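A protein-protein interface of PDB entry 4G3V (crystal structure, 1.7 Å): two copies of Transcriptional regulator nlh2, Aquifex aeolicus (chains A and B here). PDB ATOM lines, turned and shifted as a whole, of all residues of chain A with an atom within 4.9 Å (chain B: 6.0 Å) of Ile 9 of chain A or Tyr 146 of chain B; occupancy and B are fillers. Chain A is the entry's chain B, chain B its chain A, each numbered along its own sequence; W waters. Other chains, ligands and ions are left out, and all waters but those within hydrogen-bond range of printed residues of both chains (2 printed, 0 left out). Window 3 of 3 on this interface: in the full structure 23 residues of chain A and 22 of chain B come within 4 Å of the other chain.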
ATOM      1  N   LYS A   5     -14.897   6.040  -0.330  1.00  0.00           N
ATOM      2  CA  LYS A   5     -13.700   5.536   0.348  1.00  0.00           C
ATOM      3  C   LYS A   5     -12.548   6.520   0.171  1.00  0.00           C
ATOM      4  O   LYS A   5     -11.767   6.765   1.094  1.00  0.00           O
ATOM      5  CB  LYS A   5     -13.318   4.147  -0.163  1.00  0.00           C
ATOM      6  CG  LYS A   5     -14.348   3.084   0.191  1.00  0.00           C
ATOM      7  CD  LYS A   5     -13.884   1.688  -0.196  1.00  0.00           C
ATOM      8  CE  LYS A   5     -14.981   0.662   0.051  1.00  0.00           C
ATOM      9  NZ  LYS A   5     -14.593  -0.701  -0.412  1.00  0.00           N
ATOM     10  N   LEU A   6     -12.463   7.112  -1.011  1.00  0.00           N
ATOM     11  CA  LEU A   6     -11.409   8.080  -1.281  1.00  0.00           C
ATOM     12  C   LEU A   6     -11.552   9.313  -0.387  1.00  0.00           C
ATOM     13  O   LEU A   6     -10.567   9.812   0.165  1.00  0.00           O
ATOM     14  CB  LEU A   6     -11.423   8.477  -2.752  1.00  0.00           C
ATOM     15  CG  LEU A   6     -10.168   8.040  -3.505  1.00  0.00           C
ATOM     16  CD1 LEU A   6      -8.962   8.872  -3.055  1.00  0.00           C
ATOM     17  CD2 LEU A   6      -9.907   6.542  -3.304  1.00  0.00           C
ATOM     18  N   LYS A   7     -12.781   9.794  -0.235  1.00  0.00           N
ATOM     19  CA  LYS A   7     -13.050  10.918   0.649  1.00  0.00           C
ATOM     20  C   LYS A   7     -12.758  10.537   2.107  1.00  0.00           C
ATOM     21  O   LYS A   7     -12.307  11.370   2.904  1.00  0.00           O
ATOM     22  CB  LYS A   7     -14.503  11.374   0.505  1.00  0.00           C
ATOM     23  CG  LYS A   7     -14.798  12.160  -0.778  1.00  0.00           C
ATOM     24  CD  LYS A   7     -16.271  12.525  -0.864  1.00  0.00           C
ATOM     25  CE  LYS A   7     -16.606  13.192  -2.199  1.00  0.00           C
ATOM     26  NZ  LYS A   7     -18.081  13.407  -2.387  1.00  0.00           N
ATOM     27  N   GLU A   8     -13.010   9.279   2.456  1.00  0.00           N
ATOM     28  CA  GLU A   8     -12.748   8.805   3.817  1.00  0.00           C
ATOM     29  C   GLU A   8     -11.264   8.741   4.136  1.00  0.00           C
ATOM     30  O   GLU A   8     -10.848   9.106   5.218  1.00  0.00           O
ATOM     31  CB  GLU A   8     -13.368   7.426   4.052  1.00  0.00           C
ATOM     32  CG  GLU A   8     -14.883   7.433   4.025  1.00  0.00           C
ATOM     33  CD  GLU A   8     -15.482   6.044   3.937  1.00  0.00           C
ATOM     34  OE1 GLU A   8     -14.719   5.069   3.693  1.00  0.00           O
ATOM     35  OE2 GLU A   8     -16.719   5.939   4.107  1.00  0.00           O
ATOM     36  N   ILE A   9     -10.469   8.251   3.199  1.00  0.00           N
ATOM     37  CA  ILE A   9      -9.031   8.250   3.381  1.00  0.00           C
ATOM     38  C   ILE A   9      -8.523   9.675   3.579  1.00  0.00           C
ATOM     39  O   ILE A   9      -7.762   9.955   4.508  1.00  0.00           O
ATOM     40  CB  ILE A   9      -8.338   7.601   2.174  1.00  0.00           C
ATOM     41  CG1 ILE A   9      -8.557   6.084   2.205  1.00  0.00           C
ATOM     42  CG2 ILE A   9      -6.859   7.943   2.160  1.00  0.00           C
ATOM     43  CD1 ILE A   9      -8.391   5.413   0.859  1.00  0.00           C
ATOM     44  N   ASN A  10      -8.955  10.574   2.701  1.00  0.00           N
ATOM     45  CA  ASN A  10      -8.477  11.945   2.729  1.00  0.00           C
ATOM     46  C   ASN A  10      -8.889  12.683   3.979  1.00  0.00           C
ATOM     47  O   ASN A  10      -8.118  13.474   4.487  1.00  0.00           O
ATOM     48  CB  ASN A  10      -8.956  12.719   1.495  1.00  0.00           C
ATOM     49  CG  ASN A  10      -8.291  12.249   0.233  1.00  0.00           C
ATOM     50  OD1 ASN A  10      -7.154  11.776   0.259  1.00  0.00           O
ATOM     51  ND2 ASN A  10      -8.999  12.352  -0.879  1.00  0.00           N
ATOM     52  N   VAL A  11     -10.096  12.437   4.474  1.00  0.00           N
ATOM     53  CA  VAL A  11     -10.568  13.140   5.673  1.00  0.00           C
ATOM     54  C   VAL A  11      -9.831  12.662   6.924  1.00  0.00           C
ATOM     55  O   VAL A  11      -9.496  13.461   7.803  1.00  0.00           O
ATOM     56  CB  VAL A  11     -12.102  13.038   5.856  1.00  0.00           C
ATOM     57  CG1 VAL A  11     -12.508  11.684   6.402  1.00  0.00           C
ATOM     58  CG2 VAL A  11     -12.594  14.145   6.790  1.00  0.00           C
ATOM     59  N   VAL A  12      -9.537  11.369   6.993  1.00  0.00           N
ATOM     60  CA  VAL A  12      -8.711  10.839   8.082  1.00  0.00           C
ATOM     61  C   VAL A  12      -7.333  11.502   8.075  1.00  0.00           C
ATOM     62  O   VAL A  12      -6.835  11.925   9.108  1.00  0.00           O
ATOM     63  CB  VAL A  12      -8.576   9.311   8.001  1.00  0.00           C
ATOM     64  CG1 VAL A  12      -7.462   8.813   8.927  1.00  0.00           C
ATOM     65  CG2 VAL A  12      -9.896   8.669   8.372  1.00  0.00           C
ATOM     66  N   ASN A  13      -6.725  11.639   6.903  1.00  0.00           N
ATOM     67  CA  ASN A  13      -5.425  12.296   6.831  1.00  0.00           C
ATOM     68  C   ASN A  13      -5.513  13.744   7.306  1.00  0.00           C
ATOM     69  O   ASN A  13      -4.640  14.245   8.017  1.00  0.00           O
ATOM     70  CB  ASN A  13      -4.898  12.274   5.400  1.00  0.00           C
ATOM     71  CG  ASN A  13      -4.580  10.888   4.911  1.00  0.00           C
ATOM     72  OD1 ASN A  13      -4.383   9.953   5.691  1.00  0.00           O
ATOM     73  ND2 ASN A  13      -4.499  10.748   3.607  1.00  0.00           N
ATOM     74  N   PRO B  87       0.765   7.126  -0.062  1.00  0.00           N
ATOM     75  CA  PRO B  87       1.047   5.695   0.081  1.00  0.00           C
ATOM     76  C   PRO B  87       1.314   4.990  -1.239  1.00  0.00           C
ATOM     77  O   PRO B  87       0.914   5.476  -2.328  1.00  0.00           O
ATOM     78  CB  PRO B  87      -0.224   5.133   0.735  1.00  0.00           C
ATOM     79  CG  PRO B  87      -1.268   6.127   0.542  1.00  0.00           C
ATOM     80  CD  PRO B  87      -0.638   7.463   0.221  1.00  0.00           C
ATOM     81  N   LEU B  88       1.983   3.845  -1.136  1.00  0.00           N
ATOM     82  CA  LEU B  88       2.116   2.936  -2.266  1.00  0.00           C
ATOM     83  C   LEU B  88       1.607   1.543  -1.894  1.00  0.00           C
ATOM     84  O   LEU B  88       1.876   1.031  -0.801  1.00  0.00           O
ATOM     85  CB  LEU B  88       3.567   2.863  -2.740  1.00  0.00           C
ATOM     86  CG  LEU B  88       3.977   4.003  -3.681  1.00  0.00           C
ATOM     87  CD1 LEU B  88       5.490   4.014  -3.879  1.00  0.00           C
ATOM     88  CD2 LEU B  88       3.260   3.872  -5.025  1.00  0.00           C
ATOM     89  N   VAL B  89       0.891   0.941  -2.832  1.00  0.00           N
ATOM     90  CA  VAL B  89       0.324  -0.397  -2.681  1.00  0.00           C
ATOM     91  C   VAL B  89       0.801  -1.206  -3.882  1.00  0.00           C
ATOM     92  O   VAL B  89       0.336  -0.979  -5.006  1.00  0.00           O
ATOM     93  CB  VAL B  89      -1.217  -0.315  -2.669  1.00  0.00           C
ATOM     94  CG1 VAL B  89      -1.839  -1.702  -2.531  1.00  0.00           C
ATOM     95  CG2 VAL B  89      -1.673   0.621  -1.558  1.00  0.00           C
ATOM     96  N   ILE B 116       2.789  -2.793   1.196  1.00  0.00           N
ATOM     97  CA  ILE B 116       2.017  -1.569   1.417  1.00  0.00           C
ATOM     98  C   ILE B 116       2.823  -0.662   2.332  1.00  0.00           C
ATOM     99  O   ILE B 116       3.230  -1.072   3.414  1.00  0.00           O
ATOM    100  CB  ILE B 116       0.656  -1.841   2.068  1.00  0.00           C
ATOM    101  CG1 ILE B 116      -0.194  -2.732   1.168  1.00  0.00           C
ATOM    102  CG2 ILE B 116      -0.073  -0.519   2.370  1.00  0.00           C
ATOM    103  CD1 ILE B 116      -1.489  -3.173   1.805  1.00  0.00           C
ATOM    104  N   ALA B 117       3.050   0.565   1.887  1.00  0.00           N
ATOM    105  CA  ALA B 117       3.820   1.523   2.652  1.00  0.00           C
ATOM    106  C   ALA B 117       3.000   2.797   2.781  1.00  0.00           C
ATOM    107  O   ALA B 117       2.502   3.333   1.777  1.00  0.00           O
ATOM    108  CB  ALA B 117       5.158   1.791   1.977  1.00  0.00           C
ATOM    109  N   ALA B 118       2.840   3.265   4.015  1.00  0.00           N
ATOM    110  CA  ALA B 118       2.025   4.443   4.285  1.00  0.00           C
ATOM    111  C   ALA B 118       2.811   5.442   5.115  1.00  0.00           C
ATOM    112  O   ALA B 118       3.574   5.065   6.029  1.00  0.00           O
ATOM    113  CB  ALA B 118       0.753   4.061   5.013  1.00  0.00           C
ATOM    114  N   SER B 141      -9.114  -7.196  -2.452  1.00  0.00           N
ATOM    115  CA  SER B 141      -8.874  -7.277  -1.014  1.00  0.00           C
ATOM    116  C   SER B 141      -7.599  -6.529  -0.599  1.00  0.00           C
ATOM    117  O   SER B 141      -7.440  -6.142   0.556  1.00  0.00           O
ATOM    118  CB  SER B 141      -8.770  -8.742  -0.586  1.00  0.00           C
ATOM    119  OG  SER B 141      -7.743  -9.410  -1.303  1.00  0.00           O
ATOM    120  N   LEU B 142      -6.684  -6.343  -1.541  1.00  0.00           N
ATOM    121  CA  LEU B 142      -5.475  -5.581  -1.272  1.00  0.00           C
ATOM    122  C   LEU B 142      -5.827  -4.106  -1.076  1.00  0.00           C
ATOM    123  O   LEU B 142      -5.305  -3.445  -0.177  1.00  0.00           O
ATOM    124  CB  LEU B 142      -4.481  -5.757  -2.419  1.00  0.00           C
ATOM    125  CG  LEU B 142      -3.205  -4.920  -2.353  1.00  0.00           C
ATOM    126  CD1 LEU B 142      -2.487  -5.101  -1.025  1.00  0.00           C
ATOM    127  CD2 LEU B 142      -2.289  -5.300  -3.501  1.00  0.00           C
ATOM    128  N   GLU B 143      -6.730  -3.599  -1.911  1.00  0.00           N
ATOM    129  CA  GLU B 143      -7.142  -2.202  -1.826  1.00  0.00           C
ATOM    130  C   GLU B 143      -7.846  -1.904  -0.505  1.00  0.00           C
ATOM    131  O   GLU B 143      -7.642  -0.847   0.095  1.00  0.00           O
ATOM    132  CB  GLU B 143      -8.046  -1.829  -3.006  1.00  0.00           C
ATOM    133  CG  GLU B 143      -7.312  -1.752  -4.347  1.00  0.00           C
ATOM    134  CD  GLU B 143      -8.240  -1.419  -5.516  1.00  0.00           C
ATOM    135  OE1 GLU B 143      -9.324  -0.839  -5.275  1.00  0.00           O
ATOM    136  OE2 GLU B 143      -7.885  -1.741  -6.674  1.00  0.00           O
ATOM    137  N   ASN B 144      -8.664  -2.839  -0.040  1.00  0.00           N
ATOM    138  CA  ASN B 144      -9.343  -2.664   1.236  1.00  0.00           C
ATOM    139  C   ASN B 144      -8.351  -2.639   2.392  1.00  0.00           C
ATOM    140  O   ASN B 144      -8.455  -1.823   3.312  1.00  0.00           O
ATOM    141  CB  ASN B 144     -10.365  -3.778   1.454  1.00  0.00           C
ATOM    142  CG  ASN B 144     -11.052  -3.683   2.804  1.00  0.00           C
ATOM    143  OD1 ASN B 144     -11.879  -2.795   3.033  1.00  0.00           O
ATOM    144  ND2 ASN B 144     -10.720  -4.605   3.705  1.00  0.00           N
ATOM    145  N   PHE B 145      -7.374  -3.535   2.335  1.00  0.00           N
ATOM    146  CA  PHE B 145      -6.388  -3.649   3.390  1.00  0.00           C
ATOM    147  C   PHE B 145      -5.552  -2.374   3.470  1.00  0.00           C
ATOM    148  O   PHE B 145      -5.173  -1.920   4.563  1.00  0.00           O
ATOM    149  CB  PHE B 145      -5.493  -4.851   3.116  1.00  0.00           C
ATOM    150  CG  PHE B 145      -4.778  -5.355   4.322  1.00  0.00           C
ATOM    151  CD1 PHE B 145      -5.399  -6.230   5.185  1.00  0.00           C
ATOM    152  CD2 PHE B 145      -3.483  -4.973   4.581  1.00  0.00           C
ATOM    153  CE1 PHE B 145      -4.736  -6.708   6.296  1.00  0.00           C
ATOM    154  CE2 PHE B 145      -2.814  -5.437   5.689  1.00  0.00           C
ATOM    155  CZ  PHE B 145      -3.438  -6.302   6.549  1.00  0.00           C
ATOM    156  N   TYR B 146      -5.281  -1.776   2.316  1.00  0.00           N
ATOM    157  CA  TYR B 146      -4.488  -0.569   2.279  1.00  0.00           C
ATOM    158  C   TYR B 146      -5.100   0.520   3.157  1.00  0.00           C
ATOM    159  O   TYR B 146      -4.374   1.251   3.824  1.00  0.00           O
ATOM    160  CB  TYR B 146      -4.314  -0.036   0.845  1.00  0.00           C
ATOM    161  CG  TYR B 146      -4.275   1.464   0.831  1.00  0.00           C
ATOM    162  CD1 TYR B 146      -3.230   2.151   1.441  1.00  0.00           C
ATOM    163  CD2 TYR B 146      -5.299   2.202   0.253  1.00  0.00           C
ATOM    164  CE1 TYR B 146      -3.202   3.540   1.466  1.00  0.00           C
ATOM    165  CE2 TYR B 146      -5.280   3.580   0.272  1.00  0.00           C
ATOM    166  CZ  TYR B 146      -4.230   4.247   0.880  1.00  0.00           C
ATOM    167  OH  TYR B 146      -4.204   5.626   0.892  1.00  0.00           O
ATOM    168  N   GLN B 147      -6.423   0.642   3.158  1.00  0.00           N
ATOM    169  CA  GLN B 147      -7.076   1.716   3.914  1.00  0.00           C
ATOM    170  C   GLN B 147      -6.708   1.585   5.389  1.00  0.00           C
ATOM    171  O   GLN B 147      -6.414   2.576   6.078  1.00  0.00           O
ATOM    172  CB  GLN B 147      -8.604   1.678   3.728  1.00  0.00           C
ATOM    173  CG  GLN B 147      -9.341   2.905   4.311  1.00  0.00           C
ATOM    174  CD  GLN B 147     -10.836   2.969   3.943  1.00  0.00           C
ATOM    175  OE1 GLN B 147     -11.389   2.029   3.369  1.00  0.00           O
ATOM    176  NE2 GLN B 147     -11.484   4.093   4.266  1.00  0.00           N
ATOM    177  N   THR B 148      -6.706   0.355   5.876  1.00  0.00           N
ATOM    178  CA  THR B 148      -6.401   0.113   7.276  1.00  0.00           C
ATOM    179  C   THR B 148      -4.938   0.419   7.621  1.00  0.00           C
ATOM    180  O   THR B 148      -4.649   1.001   8.668  1.00  0.00           O
ATOM    181  CB  THR B 148      -6.758  -1.317   7.662  1.00  0.00           C
ATOM    182  OG1 THR B 148      -8.180  -1.456   7.633  1.00  0.00           O
ATOM    183  CG2 THR B 148      -6.268  -1.632   9.050  1.00  0.00           C
ATOM    184  N   ILE B 149      -4.004   0.065   6.746  1.00  0.00           N
ATOM    185  CA  ILE B 149      -2.614   0.426   6.996  1.00  0.00           C
ATOM    186  C   ILE B 149      -2.472   1.955   7.005  1.00  0.00           C
ATOM    187  O   ILE B 149      -1.722   2.526   7.816  1.00  0.00           O
ATOM    188  CB  ILE B 149      -1.665  -0.238   5.980  1.00  0.00           C
ATOM    189  CG1 ILE B 149      -1.791  -1.762   6.079  1.00  0.00           C
ATOM    190  CG2 ILE B 149      -0.206   0.210   6.215  1.00  0.00           C
ATOM    191  CD1 ILE B 149      -1.456  -2.323   7.436  1.00  0.00           C
ATOM    192  N   ASN B 150      -3.187   2.637   6.115  1.00  0.00           N
ATOM    193  CA  ASN B 150      -3.141   4.094   6.132  1.00  0.00           C
ATOM    194  C   ASN B 150      -3.638   4.654   7.467  1.00  0.00           C
ATOM    195  O   ASN B 150      -3.065   5.606   8.001  1.00  0.00           O
ATOM    196  CB  ASN B 150      -3.942   4.703   4.999  1.00  0.00           C
ATOM    197  CG  ASN B 150      -3.794   6.225   4.954  1.00  0.00           C
ATOM    198  OD1 ASN B 150      -2.716   6.742   4.641  1.00  0.00           O
ATOM    199  ND2 ASN B 150      -4.858   6.943   5.307  1.00  0.00           N
ATOM    200  N   VAL B 151      -4.700   4.063   8.001  1.00  0.00           N
ATOM    201  CA  VAL B 151      -5.223   4.478   9.297  1.00  0.00           C
ATOM    202  C   VAL B 151      -4.156   4.292  10.368  1.00  0.00           C
ATOM    203  O   VAL B 151      -3.949   5.166  11.204  1.00  0.00           O
ATOM    204  CB  VAL B 151      -6.474   3.682   9.691  1.00  0.00           C
ATOM    205  CG1 VAL B 151      -6.776   3.861  11.176  1.00  0.00           C
ATOM    206  CG2 VAL B 151      -7.667   4.112   8.840  1.00  0.00           C
ATOM    207  N   ASN B 154      -1.621   6.997  10.385  1.00  0.00           N
ATOM    208  CA  ASN B 154      -2.162   8.180  11.040  1.00  0.00           C
ATOM    209  C   ASN B 154      -2.157   8.088  12.576  1.00  0.00           C
ATOM    210  O   ASN B 154      -1.824   9.062  13.269  1.00  0.00           O
ATOM    211  CB  ASN B 154      -3.561   8.456  10.527  1.00  0.00           C
ATOM    212  CG  ASN B 154      -3.544   9.146   9.161  1.00  0.00           C
ATOM    213  OD1 ASN B 154      -3.312  10.337   9.078  1.00  0.00           O
ATOM    214  ND2 ASN B 154      -3.766   8.393   8.102  1.00  0.00           N
HETATM  215  O   HOH W   1      -3.426   8.517   2.103  1.00  0.00           O
HETATM  216  O   HOH W   2      -9.847   6.177   5.993  1.00  0.00           O
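Printed residues of chain B that touch a printed residue of chain A: Tyr 146, Gln 147, Asn 150 and Asn 154. Along chain B the printed residues that touch a printed residue of chain A span positions 146 to 154. Printed residues of chain A that touch a printed residue of chain B: Glu 8, Ile 9, Val 12 and Asn 13. Hydrophobic or aromatic side chains of chain A that line the printed part of chain B: Ile 9 and Val 12. Among the printed residues, 7 pairs touch across the chains. Among the printed residues, no Asp or Glu carboxylate lies within 4 Å of a Lys or Arg side-chain nitrogen of the other chain.
Tyr 146 of chain B touches Ile 9 of chain A. Ile 9 of chain A touches Gln 147 of chain B (CG1 to CG, 3.9 Å). CG2 of Ile 9 of chain A touches ND2 of Asn 150 of chain B, at 3.9 Å. Val 12 of chain A touches Asn 154 of chain B (CG1 to ND2, 3.8 Å).
The side-chain amide nitrogen (ND2) of Asn 154 of chain B lies within hydrogen-bond range of the side-chain amide oxygen (OD1) of Asn 13 of chain A, 2.9 Å away. The side-chain amide nitrogen (NE2) of Gln 147 of chain B is in hydrogen-bond range of the side-chain carboxylate (OE1) of Glu 8 of chain A, 3.4 Å away. The side-chain amide nitrogen (ND2) of Asn 150 of chain B is in hydrogen-bond range of the side-chain amide oxygen (OD1) of Asn 13 of chain A, 3.1 Å away.
The backbone carbonyl oxygen of Ile 9 of chain A sits close to the side-chain amide nitrogen of Asn 13 of chain A (3.5 Å). The side-chain amide nitrogen of Asn 154 of chain B is in hydrogen-bond range of the backbone carbonyl oxygen of Asn 150 of chain B (2.9 Å).
Ile 9 of chain A touches just these residues of chain B: Tyr 146, Gln 147 and Asn 150. Asn 10 of chain A touches none of the printed residues of chain B. Of the printed residues of chain B, Asn 13 of chain A touches Asn 150 and Asn 154. Of chain A, only Ile 9 comes within 4 Å of Tyr 146 of chain B. Of the printed residues of chain A, Gln 147 of chain B touches Glu 8 (3.4 Å) and Ile 9 (3.9 Å). Of the printed residues of chain A, Asn 150 of chain B touches Ile 9 (3.9 Å) and Asn 13 (3.1 Å). The nearest residue of chain B that does not touch Ile 9 of chain A is Asn 154 of chain B (5.6 Å). The nearest printed residue of chain A that does not touch Tyr 146 of chain B is Asn 13 of chain A (5.8 Å).
Water W1 lies within hydrogen-bond range of the side-chain amide nitrogen (ND2) of Asn 13 of chain A (2.9 Å), the side-chain amide oxygen (OD1) of Asn 150 of chain B (3.2 Å) and the side-chain hydroxyl (OH) of Tyr 146 of chain B (3.2 Å). Water W2 bridges NE2 of Gln 147 of chain B and O of Glu 8 of chain A.
No position is printed for both chains. Of the 7 pairs that touch across the chains among the printed residues, none has its exchanged pair printed and touching as well.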
